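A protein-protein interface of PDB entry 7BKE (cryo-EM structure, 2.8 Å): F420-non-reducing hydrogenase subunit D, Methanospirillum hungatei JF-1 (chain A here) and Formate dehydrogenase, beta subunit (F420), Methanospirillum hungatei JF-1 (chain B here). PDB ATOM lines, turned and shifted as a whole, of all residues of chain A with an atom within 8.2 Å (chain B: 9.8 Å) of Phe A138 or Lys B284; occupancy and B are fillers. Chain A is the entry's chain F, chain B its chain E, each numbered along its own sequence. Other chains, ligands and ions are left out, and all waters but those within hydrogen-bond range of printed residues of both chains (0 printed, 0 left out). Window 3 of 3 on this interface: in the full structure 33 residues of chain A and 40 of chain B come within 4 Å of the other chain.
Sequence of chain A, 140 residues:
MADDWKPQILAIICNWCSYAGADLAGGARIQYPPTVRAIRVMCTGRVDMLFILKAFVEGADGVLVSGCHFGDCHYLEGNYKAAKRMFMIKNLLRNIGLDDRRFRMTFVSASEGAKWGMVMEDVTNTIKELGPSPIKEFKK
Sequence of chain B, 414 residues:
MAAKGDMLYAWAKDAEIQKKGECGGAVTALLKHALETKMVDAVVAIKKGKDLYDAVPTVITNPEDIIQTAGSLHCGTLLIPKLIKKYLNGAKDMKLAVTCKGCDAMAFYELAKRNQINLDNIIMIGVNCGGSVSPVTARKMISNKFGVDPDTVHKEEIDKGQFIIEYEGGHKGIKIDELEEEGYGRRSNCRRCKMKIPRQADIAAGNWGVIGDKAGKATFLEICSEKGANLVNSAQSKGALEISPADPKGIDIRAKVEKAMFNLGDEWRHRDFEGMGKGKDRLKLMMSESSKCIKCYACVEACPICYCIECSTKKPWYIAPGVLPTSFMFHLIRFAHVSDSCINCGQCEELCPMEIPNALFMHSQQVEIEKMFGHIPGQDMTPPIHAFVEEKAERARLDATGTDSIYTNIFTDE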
ATOM      1  N   ILE A  96      -1.045  28.125  -2.617  1.00  0.00           N
ATOM      2  CA  ILE A  96      -1.848  28.402  -1.404  1.00  0.00           C
ATOM      3  C   ILE A  96      -1.721  27.147  -0.571  1.00  0.00           C
ATOM      4  O   ILE A  96      -2.324  27.095   0.484  1.00  0.00           O
ATOM      5  CB  ILE A  96      -3.317  28.762  -1.711  1.00  0.00           C
ATOM      6  CG1 ILE A  96      -4.066  27.629  -2.415  1.00  0.00           C
ATOM      7  CG2 ILE A  96      -3.417  30.074  -2.472  1.00  0.00           C
ATOM      8  CD1 ILE A  96      -5.555  27.642  -2.187  1.00  0.00           C
ATOM      9  N   GLY A  97      -0.974  26.174  -1.066  1.00  0.00           N
ATOM     10  CA  GLY A  97      -0.740  24.950  -0.292  1.00  0.00           C
ATOM     11  C   GLY A  97      -1.821  23.898  -0.374  1.00  0.00           C
ATOM     12  O   GLY A  97      -1.786  22.967   0.419  1.00  0.00           O
ATOM     13  N   LEU A  98      -2.760  24.007  -1.296  1.00  0.00           N
ATOM     14  CA  LEU A  98      -3.745  22.915  -1.461  1.00  0.00           C
ATOM     15  C   LEU A  98      -3.128  22.026  -2.515  1.00  0.00           C
ATOM     16  O   LEU A  98      -2.272  22.501  -3.257  1.00  0.00           O
ATOM     17  CB  LEU A  98      -5.103  23.461  -1.893  1.00  0.00           C
ATOM     18  CG  LEU A  98      -6.247  22.458  -1.971  1.00  0.00           C
ATOM     19  CD1 LEU A  98      -7.223  22.673  -0.831  1.00  0.00           C
ATOM     20  CD2 LEU A  98      -6.960  22.580  -3.305  1.00  0.00           C
ATOM     21  N   SER A 133     -10.503  17.088   1.658  1.00  0.00           N
ATOM     22  CA  SER A 133      -9.858  18.374   1.463  1.00  0.00           C
ATOM     23  C   SER A 133      -9.580  19.030   2.812  1.00  0.00           C
ATOM     24  O   SER A 133     -10.315  18.805   3.776  1.00  0.00           O
ATOM     25  CB  SER A 133     -10.736  19.282   0.611  1.00  0.00           C
ATOM     26  OG  SER A 133     -10.052  20.455   0.236  1.00  0.00           O
ATOM     27  N   PRO A 134      -8.516  19.825   2.924  1.00  0.00           N
ATOM     28  CA  PRO A 134      -8.204  20.448   4.215  1.00  0.00           C
ATOM     29  C   PRO A 134      -9.010  21.690   4.539  1.00  0.00           C
ATOM     30  O   PRO A 134      -9.057  22.071   5.715  1.00  0.00           O
ATOM     31  CB  PRO A 134      -6.721  20.778   4.085  1.00  0.00           C
ATOM     32  CG  PRO A 134      -6.484  20.905   2.661  1.00  0.00           C
ATOM     33  CD  PRO A 134      -7.412  19.969   1.967  1.00  0.00           C
ATOM     34  N   ILE A 135      -9.660  22.317   3.559  1.00  0.00           N
ATOM     35  CA  ILE A 135     -10.401  23.545   3.820  1.00  0.00           C
ATOM     36  C   ILE A 135     -11.520  23.292   4.823  1.00  0.00           C
ATOM     37  O   ILE A 135     -11.807  24.130   5.689  1.00  0.00           O
ATOM     38  CB  ILE A 135     -10.947  24.113   2.500  1.00  0.00           C
ATOM     39  CG1 ILE A 135      -9.813  24.303   1.503  1.00  0.00           C
ATOM     40  CG2 ILE A 135     -11.649  25.426   2.745  1.00  0.00           C
ATOM     41  CD1 ILE A 135      -8.918  25.437   1.824  1.00  0.00           C
ATOM     42  N   LYS A 136     -12.156  22.123   4.730  1.00  0.00           N
ATOM     43  CA  LYS A 136     -13.330  21.834   5.542  1.00  0.00           C
ATOM     44  C   LYS A 136     -13.004  21.834   7.030  1.00  0.00           C
ATOM     45  O   LYS A 136     -13.874  22.109   7.863  1.00  0.00           O
ATOM     46  CB  LYS A 136     -13.926  20.496   5.120  1.00  0.00           C
ATOM     47  CG  LYS A 136     -14.222  20.417   3.640  1.00  0.00           C
ATOM     48  CD  LYS A 136     -15.146  19.267   3.317  1.00  0.00           C
ATOM     49  CE  LYS A 136     -14.371  18.004   3.042  1.00  0.00           C
ATOM     50  NZ  LYS A 136     -13.660  18.082   1.745  1.00  0.00           N
ATOM     51  N   GLU A 137     -11.761  21.517   7.391  1.00  0.00           N
ATOM     52  CA  GLU A 137     -11.388  21.621   8.795  1.00  0.00           C
ATOM     53  C   GLU A 137     -10.628  22.905   9.084  1.00  0.00           C
ATOM     54  O   GLU A 137     -10.605  23.357  10.231  1.00  0.00           O
ATOM     55  CB  GLU A 137     -10.549  20.421   9.231  1.00  0.00           C
ATOM     56  CG  GLU A 137      -9.170  20.350   8.607  1.00  0.00           C
ATOM     57  CD  GLU A 137      -9.118  19.410   7.428  1.00  0.00           C
ATOM     58  OE1 GLU A 137     -10.040  19.456   6.589  1.00  0.00           O
ATOM     59  OE2 GLU A 137      -8.160  18.613   7.347  1.00  0.00           O
ATOM     60  N   PHE A 138      -9.999  23.509   8.075  1.00  0.00           N
ATOM     61  CA  PHE A 138      -9.259  24.732   8.352  1.00  0.00           C
ATOM     62  C   PHE A 138     -10.206  25.884   8.635  1.00  0.00           C
ATOM     63  O   PHE A 138      -9.840  26.817   9.355  1.00  0.00           O
ATOM     64  CB  PHE A 138      -8.344  25.108   7.191  1.00  0.00           C
ATOM     65  CG  PHE A 138      -7.192  24.166   6.977  1.00  0.00           C
ATOM     66  CD1 PHE A 138      -7.033  23.037   7.759  1.00  0.00           C
ATOM     67  CD2 PHE A 138      -6.246  24.436   6.003  1.00  0.00           C
ATOM     68  CE1 PHE A 138      -5.976  22.174   7.546  1.00  0.00           C
ATOM     69  CE2 PHE A 138      -5.183  23.586   5.800  1.00  0.00           C
ATOM     70  CZ  PHE A 138      -5.043  22.458   6.574  1.00  0.00           C
ATOM     71  N   LYS A 139     -11.414  25.845   8.072  1.00  0.00           N
ATOM     72  CA  LYS A 139     -12.391  26.898   8.328  1.00  0.00           C
ATOM     73  C   LYS A 139     -12.726  27.013   9.810  1.00  0.00           C
ATOM     74  O   LYS A 139     -12.408  28.022  10.445  1.00  0.00           O
ATOM     75  CB  LYS A 139     -13.688  26.648   7.564  1.00  0.00           C
ATOM     76  CG  LYS A 139     -13.638  26.901   6.084  1.00  0.00           C
ATOM     77  CD  LYS A 139     -14.984  26.543   5.495  1.00  0.00           C
ATOM     78  CE  LYS A 139     -14.899  26.300   4.019  1.00  0.00           C
ATOM     79  NZ  LYS A 139     -16.089  25.558   3.532  1.00  0.00           N
ATOM     80  N   LYS A 140     -13.360  25.980  10.357  1.00  0.00           N
ATOM     81  CA  LYS A 140     -13.836  25.981  11.739  1.00  0.00           C
ATOM     82  C   LYS A 140     -14.688  27.205  12.054  1.00  0.00           C
ATOM     83  O   LYS A 140     -15.188  27.881  11.154  1.00  0.00           O
ATOM     84  CB  LYS A 140     -12.659  25.900  12.715  1.00  0.00           C
ATOM     85  CG  LYS A 140     -12.085  24.509  12.886  1.00  0.00           C
ATOM     86  CD  LYS A 140     -11.020  24.494  13.961  1.00  0.00           C
ATOM     87  CE  LYS A 140     -10.462  23.100  14.163  1.00  0.00           C
ATOM     88  NZ  LYS A 140      -9.473  23.061  15.271  1.00  0.00           N
ATOM     89  N   MET B 276       7.153  31.443   4.503  1.00  0.00           N
ATOM     90  CA  MET B 276       5.657  31.335   4.532  1.00  0.00           C
ATOM     91  C   MET B 276       5.250  29.879   4.738  1.00  0.00           C
ATOM     92  O   MET B 276       4.158  29.638   5.230  1.00  0.00           O
ATOM     93  CB  MET B 276       4.976  31.804   3.244  1.00  0.00           C
ATOM     94  CG  MET B 276       5.206  33.229   2.877  1.00  0.00           C
ATOM     95  SD  MET B 276       4.313  33.541   1.349  1.00  0.00           S
ATOM     96  CE  MET B 276       2.945  32.408   1.548  1.00  0.00           C
ATOM     97  N   GLY B 277       6.115  28.948   4.370  1.00  0.00           N
ATOM     98  CA  GLY B 277       5.830  27.524   4.583  1.00  0.00           C
ATOM     99  C   GLY B 277       5.600  26.827   3.275  1.00  0.00           C
ATOM    100  O   GLY B 277       5.813  27.465   2.244  1.00  0.00           O
ATOM    101  N   LYS B 278       5.229  25.555   3.317  1.00  0.00           N
ATOM    102  CA  LYS B 278       4.951  24.758   2.103  1.00  0.00           C
ATOM    103  C   LYS B 278       3.819  23.799   2.453  1.00  0.00           C
ATOM    104  O   LYS B 278       3.698  23.458   3.631  1.00  0.00           O
ATOM    105  CB  LYS B 278       6.178  23.926   1.738  1.00  0.00           C
ATOM    106  CG  LYS B 278       7.372  24.695   1.198  1.00  0.00           C
ATOM    107  CD  LYS B 278       7.848  24.187  -0.147  1.00  0.00           C
ATOM    108  CE  LYS B 278       7.369  25.039  -1.301  1.00  0.00           C
ATOM    109  NZ  LYS B 278       6.963  24.209  -2.457  1.00  0.00           N
ATOM    110  N   GLY B 279       3.031  23.377   1.472  1.00  0.00           N
ATOM    111  CA  GLY B 279       1.964  22.390   1.707  1.00  0.00           C
ATOM    112  C   GLY B 279       0.844  22.907   2.563  1.00  0.00           C
ATOM    113  O   GLY B 279       0.565  24.082   2.468  1.00  0.00           O
ATOM    114  N   LYS B 280       0.227  22.054   3.364  1.00  0.00           N
ATOM    115  CA  LYS B 280      -0.947  22.427   4.186  1.00  0.00           C
ATOM    116  C   LYS B 280      -0.574  23.456   5.251  1.00  0.00           C
ATOM    117  O   LYS B 280      -1.491  24.114   5.738  1.00  0.00           O
ATOM    118  CB  LYS B 280      -1.672  21.171   4.670  1.00  0.00           C
ATOM    119  CG  LYS B 280      -1.621  20.902   6.168  1.00  0.00           C
ATOM    120  CD  LYS B 280      -2.694  19.944   6.636  1.00  0.00           C
ATOM    121  CE  LYS B 280      -2.171  18.560   6.942  1.00  0.00           C
ATOM    122  NZ  LYS B 280      -0.798  18.599   7.501  1.00  0.00           N
ATOM    123  N   ASP B 281       0.698  23.565   5.630  1.00  0.00           N
ATOM    124  CA  ASP B 281       1.162  24.631   6.551  1.00  0.00           C
ATOM    125  C   ASP B 281       0.961  26.012   5.932  1.00  0.00           C
ATOM    126  O   ASP B 281       0.553  26.889   6.676  1.00  0.00           O
ATOM    127  CB  ASP B 281       2.646  24.454   6.812  1.00  0.00           C
ATOM    128  CG  ASP B 281       2.953  24.216   8.278  1.00  0.00           C
ATOM    129  OD1 ASP B 281       2.117  24.607   9.112  1.00  0.00           O
ATOM    130  OD2 ASP B 281       4.019  23.645   8.571  1.00  0.00           O
ATOM    131  N   ARG B 282       1.254  26.199   4.644  1.00  0.00           N
ATOM    132  CA  ARG B 282       1.012  27.474   3.928  1.00  0.00           C
ATOM    133  C   ARG B 282      -0.482  27.750   3.882  1.00  0.00           C
ATOM    134  O   ARG B 282      -0.811  28.891   4.004  1.00  0.00           O
ATOM    135  CB  ARG B 282       1.598  27.430   2.521  1.00  0.00           C
ATOM    136  CG  ARG B 282       1.902  28.785   1.911  1.00  0.00           C
ATOM    137  CD  ARG B 282       2.399  28.504   0.518  1.00  0.00           C
ATOM    138  NE  ARG B 282       3.832  28.684   0.414  1.00  0.00           N
ATOM    139  CZ  ARG B 282       4.415  29.431  -0.508  1.00  0.00           C
ATOM    140  NH1 ARG B 282       3.677  30.067  -1.402  1.00  0.00           N
ATOM    141  NH2 ARG B 282       5.730  29.543  -0.536  1.00  0.00           N
ATOM    142  N   LEU B 283      -1.338  26.753   3.680  1.00  0.00           N
ATOM    143  CA  LEU B 283      -2.812  26.941   3.729  1.00  0.00           C
ATOM    144  C   LEU B 283      -3.246  27.349   5.128  1.00  0.00           C
ATOM    145  O   LEU B 283      -4.047  28.236   5.221  1.00  0.00           O
ATOM    146  CB  LEU B 283      -3.527  25.672   3.271  1.00  0.00           C
ATOM    147  CG  LEU B 283      -4.993  25.816   2.877  1.00  0.00           C
ATOM    148  CD1 LEU B 283      -5.210  27.022   1.985  1.00  0.00           C
ATOM    149  CD2 LEU B 283      -5.464  24.554   2.184  1.00  0.00           C
ATOM    150  N   LYS B 284      -2.721  26.747   6.179  1.00  0.00           N
ATOM    151  CA  LYS B 284      -3.093  27.245   7.519  1.00  0.00           C
ATOM    152  C   LYS B 284      -2.501  28.644   7.742  1.00  0.00           C
ATOM    153  O   LYS B 284      -3.167  29.441   8.396  1.00  0.00           O
ATOM    154  CB  LYS B 284      -2.772  26.222   8.600  1.00  0.00           C
ATOM    155  CG  LYS B 284      -3.860  26.035   9.642  1.00  0.00           C
ATOM    156  CD  LYS B 284      -4.154  24.584   9.936  1.00  0.00           C
ATOM    157  CE  LYS B 284      -3.241  24.009  10.996  1.00  0.00           C
ATOM    158  NZ  LYS B 284      -2.773  25.053  11.940  1.00  0.00           N
ATOM    159  N   LEU B 285      -1.286  28.939   7.265  1.00  0.00           N
ATOM    160  CA  LEU B 285      -0.858  30.321   7.421  1.00  0.00           C
ATOM    161  C   LEU B 285      -1.811  31.267   6.710  1.00  0.00           C
ATOM    162  O   LEU B 285      -2.322  32.220   7.312  1.00  0.00           O
ATOM    163  CB  LEU B 285       0.563  30.493   6.898  1.00  0.00           C
ATOM    164  CG  LEU B 285       1.061  31.927   6.907  1.00  0.00           C
ATOM    165  CD1 LEU B 285       1.201  32.399   8.326  1.00  0.00           C
ATOM    166  CD2 LEU B 285       2.376  32.024   6.189  1.00  0.00           C
ATOM    167  N   MET B 286      -2.086  31.003   5.432  1.00  0.00           N
ATOM    168  CA  MET B 286      -2.928  31.909   4.662  1.00  0.00           C
ATOM    169  C   MET B 286      -4.325  32.006   5.251  1.00  0.00           C
ATOM    170  O   MET B 286      -4.871  33.102   5.384  1.00  0.00           O
ATOM    171  CB  MET B 286      -3.001  31.462   3.206  1.00  0.00           C
ATOM    172  CG  MET B 286      -1.681  31.367   2.498  1.00  0.00           C
ATOM    173  SD  MET B 286      -1.884  31.885   0.795  1.00  0.00           S
ATOM    174  CE  MET B 286      -0.200  31.870   0.229  1.00  0.00           C
ATOM    175  N   MET B 287      -4.926  30.872   5.609  1.00  0.00           N
ATOM    176  CA  MET B 287      -6.309  30.914   6.064  1.00  0.00           C
ATOM    177  C   MET B 287      -6.426  31.576   7.427  1.00  0.00           C
ATOM    178  O   MET B 287      -7.338  32.378   7.653  1.00  0.00           O
ATOM    179  CB  MET B 287      -6.890  29.508   6.089  1.00  0.00           C
ATOM    180  CG  MET B 287      -7.088  28.931   4.713  1.00  0.00           C
ATOM    181  SD  MET B 287      -8.130  27.483   4.688  1.00  0.00           S
ATOM    182  CE  MET B 287      -9.727  28.231   4.928  1.00  0.00           C
ATOM    183  N   SER B 288      -5.505  31.279   8.340  1.00  0.00           N
ATOM    184  CA  SER B 288      -5.577  31.898   9.657  1.00  0.00           C
ATOM    185  C   SER B 288      -5.285  33.384   9.596  1.00  0.00           C
ATOM    186  O   SER B 288      -5.878  34.150  10.360  1.00  0.00           O
ATOM    187  CB  SER B 288      -4.619  31.210  10.620  1.00  0.00           C
ATOM    188  OG  SER B 288      -5.048  29.889  10.883  1.00  0.00           O
ATOM    189  N   GLU B 289      -4.382  33.819   8.717  1.00  0.00           N
ATOM    190  CA  GLU B 289      -4.161  35.252   8.567  1.00  0.00           C
ATOM    191  C   GLU B 289      -5.379  35.929   7.968  1.00  0.00           C
ATOM    192  O   GLU B 289      -5.876  36.920   8.505  1.00  0.00           O
ATOM    193  CB  GLU B 289      -2.933  35.518   7.713  1.00  0.00           C
ATOM    194  CG  GLU B 289      -1.657  35.112   8.376  1.00  0.00           C
ATOM    195  CD  GLU B 289      -1.376  35.919   9.606  1.00  0.00           C
ATOM    196  OE1 GLU B 289      -1.539  37.155   9.554  1.00  0.00           O
ATOM    197  OE2 GLU B 289      -1.004  35.318  10.634  1.00  0.00           O
ATOM    198  N   SER B 290      -5.890  35.396   6.865  1.00  0.00           N
ATOM    199  CA  SER B 290      -7.005  36.019   6.177  1.00  0.00           C
ATOM    200  C   SER B 290      -8.310  35.947   6.953  1.00  0.00           C
ATOM    201  O   SER B 290      -9.258  36.644   6.589  1.00  0.00           O
ATOM    202  CB  SER B 290      -7.171  35.371   4.813  1.00  0.00           C
ATOM    203  OG  SER B 290      -5.913  35.251   4.183  1.00  0.00           O
ATOM    204  N   SER B 291      -8.397  35.126   7.996  1.00  0.00           N
ATOM    205  CA  SER B 291      -9.609  35.157   8.803  1.00  0.00           C
ATOM    206  C   SER B 291      -9.744  36.444   9.599  1.00  0.00           C
ATOM    207  O   SER B 291     -10.789  36.663  10.211  1.00  0.00           O
ATOM    208  CB  SER B 291      -9.648  33.972   9.757  1.00  0.00           C
ATOM    209  OG  SER B 291      -8.686  34.117  10.783  1.00  0.00           O
ATOM    210  N   LYS B 292      -8.709  37.283   9.621  1.00  0.00           N
ATOM    211  CA  LYS B 292      -8.753  38.547  10.340  1.00  0.00           C
ATOM    212  C   LYS B 292      -9.421  39.665   9.557  1.00  0.00           C
ATOM    213  O   LYS B 292      -9.784  40.671  10.159  1.00  0.00           O
ATOM    214  CB  LYS B 292      -7.344  39.002  10.696  1.00  0.00           C
ATOM    215  CG  LYS B 292      -6.631  38.145  11.683  1.00  0.00           C
ATOM    216  CD  LYS B 292      -5.359  38.810  12.112  1.00  0.00           C
ATOM    217  CE  LYS B 292      -4.248  38.508  11.155  1.00  0.00           C
ATOM    218  NZ  LYS B 292      -3.019  39.238  11.521  1.00  0.00           N
ATOM    219  N   THR B 326     -14.980  36.659   7.465  1.00  0.00           N
ATOM    220  CA  THR B 326     -15.251  36.463   6.053  1.00  0.00           C
ATOM    221  C   THR B 326     -14.558  35.218   5.515  1.00  0.00           C
ATOM    222  O   THR B 326     -13.611  34.689   6.097  1.00  0.00           O
ATOM    223  CB  THR B 326     -14.813  37.693   5.260  1.00  0.00           C
ATOM    224  OG1 THR B 326     -15.004  37.453   3.864  1.00  0.00           O
ATOM    225  CG2 THR B 326     -13.363  37.997   5.514  1.00  0.00           C
ATOM    226  N   PHE B 328     -12.445  32.657   2.975  1.00  0.00           N
ATOM    227  CA  PHE B 328     -11.195  32.689   2.234  1.00  0.00           C
ATOM    228  C   PHE B 328     -11.418  33.071   0.783  1.00  0.00           C
ATOM    229  O   PHE B 328     -10.454  33.394   0.079  1.00  0.00           O
ATOM    230  CB  PHE B 328     -10.510  31.326   2.342  1.00  0.00           C
ATOM    231  CG  PHE B 328      -9.084  31.318   1.901  1.00  0.00           C
ATOM    232  CD1 PHE B 328      -8.569  30.231   1.232  1.00  0.00           C
ATOM    233  CD2 PHE B 328      -8.259  32.386   2.155  1.00  0.00           C
ATOM    234  CE1 PHE B 328      -7.264  30.217   0.818  1.00  0.00           C
ATOM    235  CE2 PHE B 328      -6.952  32.371   1.741  1.00  0.00           C
ATOM    236  CZ  PHE B 328      -6.456  31.287   1.071  1.00  0.00           C
ATOM    237  N   PHE B 361       1.875  37.417   0.283  1.00  0.00           N
ATOM    238  CA  PHE B 361       1.128  36.353  -0.381  1.00  0.00           C
ATOM    239  C   PHE B 361       1.060  36.593  -1.883  1.00  0.00           C
ATOM    240  O   PHE B 361       1.346  35.696  -2.693  1.00  0.00           O
ATOM    241  CB  PHE B 361      -0.277  36.265   0.200  1.00  0.00           C
ATOM    242  CG  PHE B 361      -0.320  35.955   1.664  1.00  0.00           C
ATOM    243  CD1 PHE B 361       0.754  35.375   2.301  1.00  0.00           C
ATOM    244  CD2 PHE B 361      -1.450  36.227   2.401  1.00  0.00           C
ATOM    245  CE1 PHE B 361       0.703  35.085   3.641  1.00  0.00           C
ATOM    246  CE2 PHE B 361      -1.501  35.937   3.737  1.00  0.00           C
ATOM    247  CZ  PHE B 361      -0.422  35.367   4.359  1.00  0.00           C
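Among the printed residues, merely in contact across the chains: Ile A96 with Arg B282, Gly A97 with Lys B280, Leu A98 with Leu B283, Pro A134 with Leu B283, Ile A135 with Leu B283, Ile A135 with Met B287, Phe A138 with Lys B280, Phe A138 with Leu B283, Phe A138 with Lys B284 and Phe A138 with Met B287.
The side-chain hydroxyl (OG) of Ser B288 lies within hydrogen-bond range of the backbone carbonyl oxygen (O) of Lys B284 (3.2 Å). The backbone carbonyl oxygen (O) of Gly B277 sits at hydrogen-bond distance from the guanidinium group (NE) of Arg B282, at 3.0 Å.
Of chain B, only Lys B280 (3.4 Å), Leu B283 (3.6 Å), Lys B284 (3.9 Å) and Met B287 (3.5 Å) come within 4 Å of Phe A138. Lys B284 touches one residue of chain A. Of chain B, only Leu B283 (3.8 Å) comes within 4 Å of Pro A134. Of the printed residues of chain B, Leu A98 touches Leu B283 (3.97 Å). Printed residues of chain B within 4 Å of Ile A96: Arg B282 (3.9 Å) and Leu B283 (3.3 Å). Printed residues of chain A within 4 Å of Leu B283: Ile A96, Leu A98, Pro A134, Ile A135 and Phe A138. Of the printed residues of chain B, Gly A97 touches Gly B279 and Lys B280. The nearest printed residue of chain B that does not touch Phe A138 is Asp B281 (5.9 Å). The nearest residue of chain A that does not touch Lys B284 is Ile A96 (5.7 Å). The nearest printed residue of chain B that does not touch Leu A98 is Gly B279 (5.0 Å).
O of Gly A97 sits close to O of Gly B279 (3.3 Å). The backbone carbonyl oxygen of Ile A96 lies close to the backbone NH of Leu B283 (3.4 Å).
Of the 11 printed residues of chain A, 6 touch a printed residue of chain B. Printed residues of chain B that touch a printed residue of chain A: Gly B279, Lys B280, Arg B282, Leu B283, Lys B284 and Met B287. Hydrophobic or aromatic side chains of chain B that line the printed part of chain A: Leu B283 and Met B287. Among the printed residues, no Asp or Glu carboxylate lies within 4 Å of a Lys or Arg side-chain nitrogen of the other chain.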
